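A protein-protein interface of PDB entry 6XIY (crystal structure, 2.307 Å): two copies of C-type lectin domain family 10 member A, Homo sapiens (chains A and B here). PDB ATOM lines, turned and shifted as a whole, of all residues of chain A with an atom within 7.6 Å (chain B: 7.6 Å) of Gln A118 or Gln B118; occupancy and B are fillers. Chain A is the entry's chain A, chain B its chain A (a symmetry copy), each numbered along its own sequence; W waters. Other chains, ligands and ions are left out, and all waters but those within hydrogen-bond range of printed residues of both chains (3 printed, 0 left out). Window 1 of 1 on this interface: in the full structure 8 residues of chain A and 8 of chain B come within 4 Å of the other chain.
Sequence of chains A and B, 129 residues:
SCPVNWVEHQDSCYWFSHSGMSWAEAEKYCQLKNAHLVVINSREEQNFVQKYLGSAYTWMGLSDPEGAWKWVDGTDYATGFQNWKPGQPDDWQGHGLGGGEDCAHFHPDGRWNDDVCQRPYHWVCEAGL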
ATOM      1  N   GLY A  20      17.163  23.661  22.389  1.00  0.00           N
ATOM      2  CA  GLY A  20      18.553  23.848  22.831  1.00  0.00           C
ATOM      3  C   GLY A  20      19.509  23.795  21.663  1.00  0.00           C
ATOM      4  O   GLY A  20      19.253  23.041  20.713  1.00  0.00           O
ATOM      5  N   MET A  21      20.588  24.554  21.763  1.00  0.00           N
ATOM      6  CA  MET A  21      21.627  24.734  20.716  1.00  0.00           C
ATOM      7  C   MET A  21      22.912  25.167  21.410  1.00  0.00           C
ATOM      8  O   MET A  21      22.809  25.816  22.449  1.00  0.00           O
ATOM      9  CB  MET A  21      21.232  25.854  19.759  1.00  0.00           C
ATOM     10  CG  MET A  21      20.242  25.451  18.676  1.00  0.00           C
ATOM     11  SD  MET A  21      20.095  26.806  17.456  1.00  0.00           S
ATOM     12  CE  MET A  21      18.754  26.196  16.428  1.00  0.00           C
ATOM     13  N   SER A  22      24.063  24.876  20.825  1.00  0.00           N
ATOM     14  CA  SER A  22      25.367  25.455  21.213  1.00  0.00           C
ATOM     15  C   SER A  22      25.256  26.975  21.168  1.00  0.00           C
ATOM     16  O   SER A  22      24.380  27.491  20.473  1.00  0.00           O
ATOM     17  CB  SER A  22      26.471  25.001  20.299  1.00  0.00           C
ATOM     18  OG  SER A  22      26.233  25.454  18.978  1.00  0.00           O
ATOM     19  N   TRP A  23      26.143  27.654  21.876  1.00  0.00           N
ATOM     20  CA  TRP A  23      26.162  29.121  21.906  1.00  0.00           C
ATOM     21  C   TRP A  23      26.330  29.671  20.486  1.00  0.00           C
ATOM     22  O   TRP A  23      25.640  30.642  20.166  1.00  0.00           O
ATOM     23  CB  TRP A  23      27.223  29.606  22.880  1.00  0.00           C
ATOM     24  CG  TRP A  23      27.142  31.071  23.170  1.00  0.00           C
ATOM     25  CD1 TRP A  23      26.540  31.681  24.241  1.00  0.00           C
ATOM     26  CD2 TRP A  23      27.745  32.113  22.386  1.00  0.00           C
ATOM     27  NE1 TRP A  23      26.720  33.037  24.173  1.00  0.00           N
ATOM     28  CE2 TRP A  23      27.449  33.333  23.043  1.00  0.00           C
ATOM     29  CE3 TRP A  23      28.477  32.132  21.187  1.00  0.00           C
ATOM     30  CZ2 TRP A  23      27.875  34.555  22.534  1.00  0.00           C
ATOM     31  CZ3 TRP A  23      28.883  33.351  20.677  1.00  0.00           C
ATOM     32  CH2 TRP A  23      28.581  34.544  21.343  1.00  0.00           C
ATOM     33  N   ALA A  24      27.182  29.077  19.651  1.00  0.00           N
ATOM     34  CA  ALA A  24      27.462  29.604  18.295  1.00  0.00           C
ATOM     35  C   ALA A  24      26.213  29.430  17.417  1.00  0.00           C
ATOM     36  O   ALA A  24      25.884  30.373  16.685  1.00  0.00           O
ATOM     37  CB  ALA A  24      28.680  28.936  17.688  1.00  0.00           C
ATOM     38  N   GLU A  25      25.536  28.284  17.494  1.00  0.00           N
ATOM     39  CA  GLU A  25      24.329  28.011  16.666  1.00  0.00           C
ATOM     40  C   GLU A  25      23.211  28.949  17.108  1.00  0.00           C
ATOM     41  O   GLU A  25      22.511  29.497  16.234  1.00  0.00           O
ATOM     42  CB  GLU A  25      23.908  26.546  16.756  1.00  0.00           C
ATOM     43  CG  GLU A  25      24.913  25.608  16.095  1.00  0.00           C
ATOM     44  CD  GLU A  25      24.929  25.633  14.567  1.00  0.00           C
ATOM     45  OE1 GLU A  25      23.845  25.764  13.957  1.00  0.00           O
ATOM     46  OE2 GLU A  25      26.032  25.517  13.980  1.00  0.00           O
ATOM     47  N   TRP A  59      21.257  30.323  27.386  1.00  0.00           N
ATOM     48  CA  TRP A  59      22.342  31.198  26.864  1.00  0.00           C
ATOM     49  C   TRP A  59      21.921  32.677  26.846  1.00  0.00           C
ATOM     50  O   TRP A  59      20.789  32.972  26.473  1.00  0.00           O
ATOM     51  CB  TRP A  59      22.757  30.767  25.455  1.00  0.00           C
ATOM     52  CG  TRP A  59      23.454  29.447  25.331  1.00  0.00           C
ATOM     53  CD1 TRP A  59      23.134  28.452  24.458  1.00  0.00           C
ATOM     54  CD2 TRP A  59      24.613  28.984  26.038  1.00  0.00           C
ATOM     55  NE1 TRP A  59      24.002  27.398  24.578  1.00  0.00           N
ATOM     56  CE2 TRP A  59      24.918  27.690  25.542  1.00  0.00           C
ATOM     57  CE3 TRP A  59      25.432  29.517  27.024  1.00  0.00           C
ATOM     58  CZ2 TRP A  59      25.998  26.939  25.995  1.00  0.00           C
ATOM     59  CZ3 TRP A  59      26.477  28.753  27.508  1.00  0.00           C
ATOM     60  CH2 TRP A  59      26.760  27.489  26.991  1.00  0.00           C
ATOM     61  N   HIS A  95      35.643  19.664  33.722  1.00  0.00           N
ATOM     62  CA  HIS A  95      34.727  18.918  32.817  1.00  0.00           C
ATOM     63  C   HIS A  95      35.539  17.977  31.907  1.00  0.00           C
ATOM     64  O   HIS A  95      34.975  16.971  31.465  1.00  0.00           O
ATOM     65  CB  HIS A  95      33.845  19.900  32.025  1.00  0.00           C
ATOM     66  CG  HIS A  95      34.612  20.949  31.295  1.00  0.00           C
ATOM     67  ND1 HIS A  95      35.400  20.659  30.202  1.00  0.00           N
ATOM     68  CD2 HIS A  95      34.736  22.272  31.510  1.00  0.00           C
ATOM     69  CE1 HIS A  95      35.950  21.765  29.750  1.00  0.00           C
ATOM     70  NE2 HIS A  95      35.547  22.775  30.529  1.00  0.00           N
ATOM     71  N   LEU A  97      36.538  18.327  28.898  1.00  0.00           N
ATOM     72  CA  LEU A  97      36.052  18.464  27.495  1.00  0.00           C
ATOM     73  C   LEU A  97      37.049  19.270  26.666  1.00  0.00           C
ATOM     74  O   LEU A  97      36.816  19.397  25.471  1.00  0.00           O
ATOM     75  CB  LEU A  97      34.696  19.177  27.492  1.00  0.00           C
ATOM     76  CG  LEU A  97      33.433  18.316  27.561  1.00  0.00           C
ATOM     77  CD1 LEU A  97      33.686  16.909  28.071  1.00  0.00           C
ATOM     78  CD2 LEU A  97      32.344  19.020  28.359  1.00  0.00           C
ATOM     79  N   GLY A  98      38.082  19.845  27.296  1.00  0.00           N
ATOM     80  CA  GLY A  98      39.077  20.692  26.615  1.00  0.00           C
ATOM     81  C   GLY A  98      38.765  22.166  26.789  1.00  0.00           C
ATOM     82  O   GLY A  98      37.574  22.555  26.610  1.00  0.00           O
ATOM     83  N   GLY A 100      38.545  25.908  28.990  1.00  0.00           N
ATOM     84  CA  GLY A 100      37.812  26.308  30.204  1.00  0.00           C
ATOM     85  C   GLY A 100      36.326  26.426  29.916  1.00  0.00           C
ATOM     86  O   GLY A 100      35.718  25.443  29.423  1.00  0.00           O
ATOM     87  N   CYS A 103      31.331  30.857  27.717  1.00  0.00           N
ATOM     88  CA  CYS A 103      29.945  31.267  27.370  1.00  0.00           C
ATOM     89  C   CYS A 103      29.101  31.311  28.645  1.00  0.00           C
ATOM     90  O   CYS A 103      29.255  30.395  29.461  1.00  0.00           O
ATOM     91  CB  CYS A 103      29.362  30.299  26.348  1.00  0.00           C
ATOM     92  SG  CYS A 103      30.130  30.441  24.709  1.00  0.00           S
ATOM     93  N   ASP A 115      30.123  28.442  31.163  1.00  0.00           N
ATOM     94  CA  ASP A 115      29.998  27.013  30.782  1.00  0.00           C
ATOM     95  C   ASP A 115      30.591  26.849  29.388  1.00  0.00           C
ATOM     96  O   ASP A 115      30.995  27.882  28.750  1.00  0.00           O
ATOM     97  CB  ASP A 115      28.542  26.511  30.851  1.00  0.00           C
ATOM     98  CG  ASP A 115      28.370  25.067  31.336  1.00  0.00           C
ATOM     99  OD1 ASP A 115      29.265  24.233  31.062  1.00  0.00           O
ATOM    100  OD2 ASP A 115      27.340  24.775  31.991  1.00  0.00           O
ATOM    101  N   VAL A 116      30.638  25.590  28.977  1.00  0.00           N
ATOM    102  CA  VAL A 116      31.216  25.095  27.703  1.00  0.00           C
ATOM    103  C   VAL A 116      30.222  25.467  26.612  1.00  0.00           C
ATOM    104  O   VAL A 116      29.047  25.071  26.724  1.00  0.00           O
ATOM    105  CB  VAL A 116      31.471  23.581  27.788  1.00  0.00           C
ATOM    106  CG1 VAL A 116      31.998  23.018  26.474  1.00  0.00           C
ATOM    107  CG2 VAL A 116      32.421  23.264  28.937  1.00  0.00           C
ATOM    108  N   CYS A 117      30.696  26.240  25.644  1.00  0.00           N
ATOM    109  CA  CYS A 117      29.912  26.843  24.535  1.00  0.00           C
ATOM    110  C   CYS A 117      29.195  25.766  23.708  1.00  0.00           C
ATOM    111  O   CYS A 117      28.159  26.086  23.127  1.00  0.00           O
ATOM    112  CB  CYS A 117      30.848  27.696  23.678  1.00  0.00           C
ATOM    113  SG  CYS A 117      31.616  29.057  24.614  1.00  0.00           S
ATOM    114  N   GLN A 118      29.751  24.557  23.642  1.00  0.00           N
ATOM    115  CA  GLN A 118      29.206  23.492  22.756  1.00  0.00           C
ATOM    116  C   GLN A 118      27.916  22.917  23.371  1.00  0.00           C
ATOM    117  O   GLN A 118      27.138  22.300  22.631  1.00  0.00           O
ATOM    118  CB  GLN A 118      30.277  22.430  22.486  1.00  0.00           C
ATOM    119  CG  GLN A 118      31.386  22.898  21.542  1.00  0.00           C
ATOM    120  CD  GLN A 118      32.310  23.954  22.111  1.00  0.00           C
ATOM    121  OE1 GLN A 118      32.571  24.996  21.498  1.00  0.00           O
ATOM    122  NE2 GLN A 118      32.829  23.693  23.297  1.00  0.00           N
ATOM    123  N   ARG A 119      27.661  23.142  24.664  1.00  0.00           N
ATOM    124  CA  ARG A 119      26.471  22.564  25.356  1.00  0.00           C
ATOM    125  C   ARG A 119      25.173  23.030  24.703  1.00  0.00           C
ATOM    126  O   ARG A 119      25.019  24.211  24.429  1.00  0.00           O
ATOM    127  CB  ARG A 119      26.501  22.938  26.838  1.00  0.00           C
ATOM    128  CG  ARG A 119      27.545  22.152  27.627  1.00  0.00           C
ATOM    129  CD  ARG A 119      27.170  22.012  29.095  1.00  0.00           C
ATOM    130  NE  ARG A 119      28.345  21.728  29.901  1.00  0.00           N
ATOM    131  CZ  ARG A 119      28.926  20.543  29.993  1.00  0.00           C
ATOM    132  NH1 ARG A 119      28.407  19.488  29.384  1.00  0.00           N
ATOM    133  NH2 ARG A 119      30.035  20.421  30.696  1.00  0.00           N
ATOM    134  N   PRO A 120      24.199  22.129  24.420  1.00  0.00           N
ATOM    135  CA  PRO A 120      22.893  22.548  23.933  1.00  0.00           C
ATOM    136  C   PRO A 120      21.996  23.077  25.064  1.00  0.00           C
ATOM    137  O   PRO A 120      21.525  22.325  25.859  1.00  0.00           O
ATOM    138  CB  PRO A 120      22.360  21.277  23.261  1.00  0.00           C
ATOM    139  CG  PRO A 120      22.955  20.155  24.063  1.00  0.00           C
ATOM    140  CD  PRO A 120      24.316  20.661  24.506  1.00  0.00           C
ATOM    141  N   TYR A 121      21.805  24.394  25.111  1.00  0.00           N
ATOM    142  CA  TYR A 121      20.991  25.094  26.133  1.00  0.00           C
ATOM    143  C   TYR A 121      19.909  25.919  25.429  1.00  0.00           C
ATOM    144  O   TYR A 121      20.021  26.209  24.219  1.00  0.00           O
ATOM    145  CB  TYR A 121      21.877  26.017  26.979  1.00  0.00           C
ATOM    146  CG  TYR A 121      22.770  25.381  28.018  1.00  0.00           C
ATOM    147  CD1 TYR A 121      22.597  24.078  28.444  1.00  0.00           C
ATOM    148  CD2 TYR A 121      23.768  26.123  28.625  1.00  0.00           C
ATOM    149  CE1 TYR A 121      23.401  23.523  29.428  1.00  0.00           C
ATOM    150  CE2 TYR A 121      24.577  25.588  29.618  1.00  0.00           C
ATOM    151  CZ  TYR A 121      24.391  24.280  30.027  1.00  0.00           C
ATOM    152  OH  TYR A 121      25.172  23.732  31.010  1.00  0.00           O
ATOM    153  N   GLY B  20      35.890  16.750  24.221  1.00  0.00           N
ATOM    154  CA  GLY B  20      34.467  16.516  23.933  1.00  0.00           C
ATOM    155  C   GLY B  20      34.016  17.305  22.729  1.00  0.00           C
ATOM    156  O   GLY B  20      34.519  18.420  22.521  1.00  0.00           O
ATOM    157  N   MET B  21      33.073  16.746  21.989  1.00  0.00           N
ATOM    158  CA  MET B  21      32.527  17.288  20.717  1.00  0.00           C
ATOM    159  C   MET B  21      31.136  16.699  20.524  1.00  0.00           C
ATOM    160  O   MET B  21      30.918  15.583  20.990  1.00  0.00           O
ATOM    161  CB  MET B  21      33.377  16.833  19.534  1.00  0.00           C
ATOM    162  CG  MET B  21      34.645  17.643  19.309  1.00  0.00           C
ATOM    163  SD  MET B  21      35.392  17.166  17.710  1.00  0.00           S
ATOM    164  CE  MET B  21      36.939  18.077  17.768  1.00  0.00           C
ATOM    165  N   SER B  22      30.259  17.393  19.815  1.00  0.00           N
ATOM    166  CA  SER B  22      28.981  16.851  19.305  1.00  0.00           C
ATOM    167  C   SER B  22      29.277  15.600  18.484  1.00  0.00           C
ATOM    168  O   SER B  22      30.401  15.449  18.008  1.00  0.00           O
ATOM    169  CB  SER B  22      28.253  17.853  18.454  1.00  0.00           C
ATOM    170  OG  SER B  22      29.016  18.170  17.304  1.00  0.00           O
ATOM    171  N   TRP B  23      28.274  14.753  18.316  1.00  0.00           N
ATOM    172  CA  TRP B  23      28.416  13.521  17.532  1.00  0.00           C
ATOM    173  C   TRP B  23      28.854  13.858  16.104  1.00  0.00           C
ATOM    174  O   TRP B  23      29.721  13.145  15.591  1.00  0.00           O
ATOM    175  CB  TRP B  23      27.133  12.710  17.605  1.00  0.00           C
ATOM    176  CG  TRP B  23      27.269  11.327  17.054  1.00  0.00           C
ATOM    177  CD1 TRP B  23      27.495  10.167  17.752  1.00  0.00           C
ATOM    178  CD2 TRP B  23      27.126  10.959  15.674  1.00  0.00           C
ATOM    179  NE1 TRP B  23      27.512   9.098  16.894  1.00  0.00           N
ATOM    180  CE2 TRP B  23      27.295   9.552  15.613  1.00  0.00           C
ATOM    181  CE3 TRP B  23      26.901  11.680  14.489  1.00  0.00           C
ATOM    182  CZ2 TRP B  23      27.235   8.864  14.406  1.00  0.00           C
ATOM    183  CZ3 TRP B  23      26.858  10.993  13.292  1.00  0.00           C
ATOM    184  CH2 TRP B  23      27.026   9.604  13.254  1.00  0.00           C
ATOM    185  N   ALA B  24      28.312  14.904  15.482  1.00  0.00           N
ATOM    186  CA  ALA B  24      28.620  15.238  14.073  1.00  0.00           C
ATOM    187  C   ALA B  24      30.077  15.716  13.972  1.00  0.00           C
ATOM    188  O   ALA B  24      30.762  15.293  13.032  1.00  0.00           O
ATOM    189  CB  ALA B  24      27.647  16.265  13.526  1.00  0.00           C
ATOM    190  N   GLU B  25      30.538  16.547  14.907  1.00  0.00           N
ATOM    191  CA  GLU B  25      31.926  17.086  14.883  1.00  0.00           C
ATOM    192  C   GLU B  25      32.900  15.935  15.121  1.00  0.00           C
ATOM    193  O   GLU B  25      33.934  15.876  14.424  1.00  0.00           O
ATOM    194  CB  GLU B  25      32.111  18.205  15.905  1.00  0.00           C
ATOM    195  CG  GLU B  25      31.323  19.460  15.545  1.00  0.00           C
ATOM    196  CD  GLU B  25      31.880  20.274  14.377  1.00  0.00           C
ATOM    197  OE1 GLU B  25      33.121  20.371  14.252  1.00  0.00           O
ATOM    198  OE2 GLU B  25      31.069  20.818  13.589  1.00  0.00           O
ATOM    199  N   TRP B  59      31.031   8.969  22.822  1.00  0.00           N
ATOM    200  CA  TRP B  59      30.328   8.652  21.548  1.00  0.00           C
ATOM    201  C   TRP B  59      30.894   7.385  20.886  1.00  0.00           C
ATOM    202  O   TRP B  59      32.110   7.212  20.866  1.00  0.00           O
ATOM    203  CB  TRP B  59      30.421   9.826  20.570  1.00  0.00           C
ATOM    204  CG  TRP B  59      29.672  11.071  20.937  1.00  0.00           C
ATOM    205  CD1 TRP B  59      30.176  12.335  20.942  1.00  0.00           C
ATOM    206  CD2 TRP B  59      28.288  11.204  21.289  1.00  0.00           C
ATOM    207  NE1 TRP B  59      29.210  13.246  21.283  1.00  0.00           N
ATOM    208  CE2 TRP B  59      28.042  12.585  21.507  1.00  0.00           C
ATOM    209  CE3 TRP B  59      27.229  10.319  21.435  1.00  0.00           C
ATOM    210  CZ2 TRP B  59      26.792  13.087  21.855  1.00  0.00           C
ATOM    211  CZ3 TRP B  59      25.998  10.812  21.825  1.00  0.00           C
ATOM    212  CH2 TRP B  59      25.783  12.175  22.019  1.00  0.00           C
ATOM    213  N   HIS B  95      14.191  16.036  28.033  1.00  0.00           N
ATOM    214  CA  HIS B  95      15.285  17.042  28.099  1.00  0.00           C
ATOM    215  C   HIS B  95      14.767  18.415  27.627  1.00  0.00           C
ATOM    216  O   HIS B  95      15.334  19.425  28.052  1.00  0.00           O
ATOM    217  CB  HIS B  95      16.505  16.556  27.298  1.00  0.00           C
ATOM    218  CG  HIS B  95      16.192  16.172  25.894  1.00  0.00           C
ATOM    219  ND1 HIS B  95      15.841  17.099  24.936  1.00  0.00           N
ATOM    220  CD2 HIS B  95      16.151  14.970  25.287  1.00  0.00           C
ATOM    221  CE1 HIS B  95      15.630  16.491  23.789  1.00  0.00           C
ATOM    222  NE2 HIS B  95      15.828  15.181  23.975  1.00  0.00           N
ATOM    223  N   LEU B  97      15.008  19.878  24.803  1.00  0.00           N
ATOM    224  CA  LEU B  97      15.994  20.474  23.855  1.00  0.00           C
ATOM    225  C   LEU B  97      15.477  20.371  22.422  1.00  0.00           C
ATOM    226  O   LEU B  97      16.152  20.889  21.541  1.00  0.00           O
ATOM    227  CB  LEU B  97      17.325  19.725  23.970  1.00  0.00           C
ATOM    228  CG  LEU B  97      18.364  20.257  24.960  1.00  0.00           C
ATOM    229  CD1 LEU B  97      17.778  21.176  26.016  1.00  0.00           C
ATOM    230  CD2 LEU B  97      19.151  19.111  25.582  1.00  0.00           C
ATOM    231  N   GLY B  98      14.358  19.669  22.198  1.00  0.00           N
ATOM    232  CA  GLY B  98      13.794  19.452  20.854  1.00  0.00           C
ATOM    233  C   GLY B  98      14.187  18.098  20.297  1.00  0.00           C
ATOM    234  O   GLY B  98      15.395  17.734  20.394  1.00  0.00           O
ATOM    235  N   GLY B 100      14.004  13.765  19.994  1.00  0.00           N
ATOM    236  CA  GLY B 100      14.273  12.686  20.962  1.00  0.00           C
ATOM    237  C   GLY B 100      15.762  12.572  21.234  1.00  0.00           C
ATOM    238  O   GLY B 100      16.391  13.587  21.626  1.00  0.00           O
ATOM    239  N   CYS B 103      21.694   9.512  19.029  1.00  0.00           N
ATOM    240  CA  CYS B 103      23.147   9.200  19.061  1.00  0.00           C
ATOM    241  C   CYS B 103      23.454   8.371  20.309  1.00  0.00           C
ATOM    242  O   CYS B 103      22.903   8.706  21.363  1.00  0.00           O
ATOM    243  CB  CYS B 103      23.952  10.494  19.037  1.00  0.00           C
ATOM    244  SG  CYS B 103      23.872  11.357  17.442  1.00  0.00           S
ATOM    245  N   ASP B 115      21.243   9.501  23.383  1.00  0.00           N
ATOM    246  CA  ASP B 115      21.335  10.881  23.922  1.00  0.00           C
ATOM    247  C   ASP B 115      21.289  11.845  22.743  1.00  0.00           C
ATOM    248  O   ASP B 115      21.274  11.382  21.550  1.00  0.00           O
ATOM    249  CB  ASP B 115      22.592  11.091  24.789  1.00  0.00           C
ATOM    250  CG  ASP B 115      22.402  12.006  26.004  1.00  0.00           C
ATOM    251  OD1 ASP B 115      21.583  12.951  25.920  1.00  0.00           O
ATOM    252  OD2 ASP B 115      23.072  11.773  27.038  1.00  0.00           O
ATOM    253  N   VAL B 116      21.252  13.119  23.103  1.00  0.00           N
ATOM    254  CA  VAL B 116      21.138  14.292  22.199  1.00  0.00           C
ATOM    255  C   VAL B 116      22.502  14.463  21.547  1.00  0.00           C
ATOM    256  O   VAL B 116      23.496  14.594  22.285  1.00  0.00           O
ATOM    257  CB  VAL B 116      20.695  15.533  22.993  1.00  0.00           C
ATOM    258  CG1 VAL B 116      20.635  16.777  22.117  1.00  0.00           C
ATOM    259  CG2 VAL B 116      19.356  15.279  23.675  1.00  0.00           C
ATOM    260  N   CYS B 117      22.515  14.402  20.223  1.00  0.00           N
ATOM    261  CA  CYS B 117      23.720  14.415  19.353  1.00  0.00           C
ATOM    262  C   CYS B 117      24.563  15.677  19.585  1.00  0.00           C
ATOM    263  O   CYS B 117      25.771  15.607  19.359  1.00  0.00           O
ATOM    264  CB  CYS B 117      23.276  14.282  17.895  1.00  0.00           C
ATOM    265  SG  CYS B 117      22.378  12.730  17.571  1.00  0.00           S
ATOM    266  N   GLN B 118      23.936  16.782  19.986  1.00  0.00           N
ATOM    267  CA  GLN B 118      24.645  18.086  20.104  1.00  0.00           C
ATOM    268  C   GLN B 118      25.537  18.078  21.360  1.00  0.00           C
ATOM    269  O   GLN B 118      26.457  18.904  21.430  1.00  0.00           O
ATOM    270  CB  GLN B 118      23.636  19.239  20.082  1.00  0.00           C
ATOM    271  CG  GLN B 118      23.021  19.492  18.704  1.00  0.00           C
ATOM    272  CD  GLN B 118      22.080  18.412  18.212  1.00  0.00           C
ATOM    273  OE1 GLN B 118      22.188  17.912  17.086  1.00  0.00           O
ATOM    274  NE2 GLN B 118      21.130  18.044  19.052  1.00  0.00           N
ATOM    275  N   ARG B 119      25.317  17.158  22.304  1.00  0.00           N
ATOM    276  CA  ARG B 119      26.087  17.123  23.582  1.00  0.00           C
ATOM    277  C   ARG B 119      27.580  16.941  23.320  1.00  0.00           C
ATOM    278  O   ARG B 119      27.960  16.092  22.529  1.00  0.00           O
ATOM    279  CB  ARG B 119      25.552  16.009  24.480  1.00  0.00           C
ATOM    280  CG  ARG B 119      24.205  16.353  25.112  1.00  0.00           C
ATOM    281  CD  ARG B 119      23.987  15.625  26.432  1.00  0.00           C
ATOM    282  NE  ARG B 119      22.573  15.558  26.755  1.00  0.00           N
ATOM    283  CZ  ARG B 119      21.866  16.559  27.253  1.00  0.00           C
ATOM    284  NH1 ARG B 119      22.449  17.708  27.562  1.00  0.00           N
ATOM    285  NH2 ARG B 119      20.569  16.406  27.435  1.00  0.00           N
ATOM    286  N   PRO B 120      28.478  17.731  23.962  1.00  0.00           N
ATOM    287  CA  PRO B 120      29.910  17.497  23.854  1.00  0.00           C
ATOM    288  C   PRO B 120      30.377  16.338  24.750  1.00  0.00           C
ATOM    289  O   PRO B 120      30.427  16.474  25.931  1.00  0.00           O
ATOM    290  CB  PRO B 120      30.504  18.857  24.240  1.00  0.00           C
ATOM    291  CG  PRO B 120      29.528  19.421  25.232  1.00  0.00           C
ATOM    292  CD  PRO B 120      28.168  18.917  24.783  1.00  0.00           C
ATOM    293  N   TYR B 121      30.687  15.197  24.139  1.00  0.00           N
ATOM    294  CA  TYR B 121      31.137  13.964  24.828  1.00  0.00           C
ATOM    295  C   TYR B 121      32.491  13.537  24.252  1.00  0.00           C
ATOM    296  O   TYR B 121      32.872  13.968  23.144  1.00  0.00           O
ATOM    297  CB  TYR B 121      30.114  12.839  24.631  1.00  0.00           C
ATOM    298  CG  TYR B 121      28.831  12.905  25.425  1.00  0.00           C
ATOM    299  CD1 TYR B 121      28.680  13.734  26.520  1.00  0.00           C
ATOM    300  CD2 TYR B 121      27.771  12.073  25.106  1.00  0.00           C
ATOM    301  CE1 TYR B 121      27.509  13.753  27.262  1.00  0.00           C
ATOM    302  CE2 TYR B 121      26.595  12.071  25.842  1.00  0.00           C
ATOM    303  CZ  TYR B 121      26.462  12.912  26.931  1.00  0.00           C
ATOM    304  OH  TYR B 121      25.314  12.922  27.677  1.00  0.00           O
HETATM  305  O   HOH W   1      29.481  16.768  28.662  1.00  0.00           O
HETATM  306  O   HOH W   2      27.180  21.161  20.232  1.00  0.00           O
HETATM  307  O   HOH W   3      21.413  20.484  28.103  1.00  0.00           O
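The backbone NH of Gly A20 lies within hydrogen-bond range of the backbone carbonyl oxygen of Leu B97 (3.1 Å). The backbone carbonyl oxygen (O) of Leu A97 is in hydrogen-bond range of the backbone NH (N) of Gly B20, 3.1 Å away.
A ring nitrogen (ND1) of His A95 is in hydrogen-bond range of the backbone NH of Leu A97. ND1 of His B95 is in hydrogen-bond range of N of Leu B97 (2.9 Å). SG of Cys A117 forms a disulfide with SG of Cys A103 (2.0 Å). The side-chain sulfur (SG) of Cys B103 is disulfide-bonded to the side-chain sulfur (SG) of Cys B117, at 2.0 Å.
O of Pro B120 touches CG of Leu A97, 3.9 Å away. Gln A118 touches Gln B118 (O to O, 3.7 Å). CB of Gln A118 touches CB of Pro B120, 3.99 Å away. Pro A120 touches Leu B97. Pro A120 touches Gln B118 (CB to CB, 3.99 Å).
Of the printed residues of chain B, Gln A118 touches Gln B118 and Pro B120. Printed residues of chain B within 4 Å of Pro A120: Leu B97 (3.9 Å) and Gln B118 (3.99 Å). Tyr A121 touches none of the printed residues of chain B. Cys B117 touches none of the printed residues of chain A. Printed residues of chain A within 4 Å of Gln B118: Gln A118 (3.7 Å) and Pro A120 (3.99 Å). Of the printed residues of chain A, Pro B120 touches Leu A97 (3.9 Å) and Gln A118 (3.99 Å). The nearest printed residue of chain B that does not touch Gln A118 is Arg B119 (5.4 Å). The nearest printed residue of chain A that does not touch Gln B118 is Arg A119 (5.4 Å). The nearest printed residue of chain A that does not touch Leu B97 is Tyr A121 (5.1 Å).
Of the 19 printed residues of chain A, 4 touch a printed residue of chain B. Hydrophobic or aromatic side chains of chain B that line the printed part of chain A: Leu B97 and Pro B120.
Gly A20 touches Leu B97, and with the chains exchanged Leu A97 touches Gly B20. Leu A97 touches Pro B120, and with the chains exchanged Pro A120 touches Leu B97. Gln A118 touches its own counterpart, Gln B118. Gln A118 touches Pro B120, and with the chains exchanged Pro A120 touches Gln B118.
Water W2 bridges the backbone carbonyl oxygen of Gln A118 (2.7 Å) and the backbone carbonyl oxygen of Gln B118 (2.7 Å). Water W3 bridges the backbone carbonyl oxygen of Pro A120 (2.9 Å) and the guanidinium group of Arg B119 (3.0 Å). Water W1 bridges the backbone carbonyl oxygen (O) of Pro B120 and the guanidinium group (NH1) of Arg A119.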
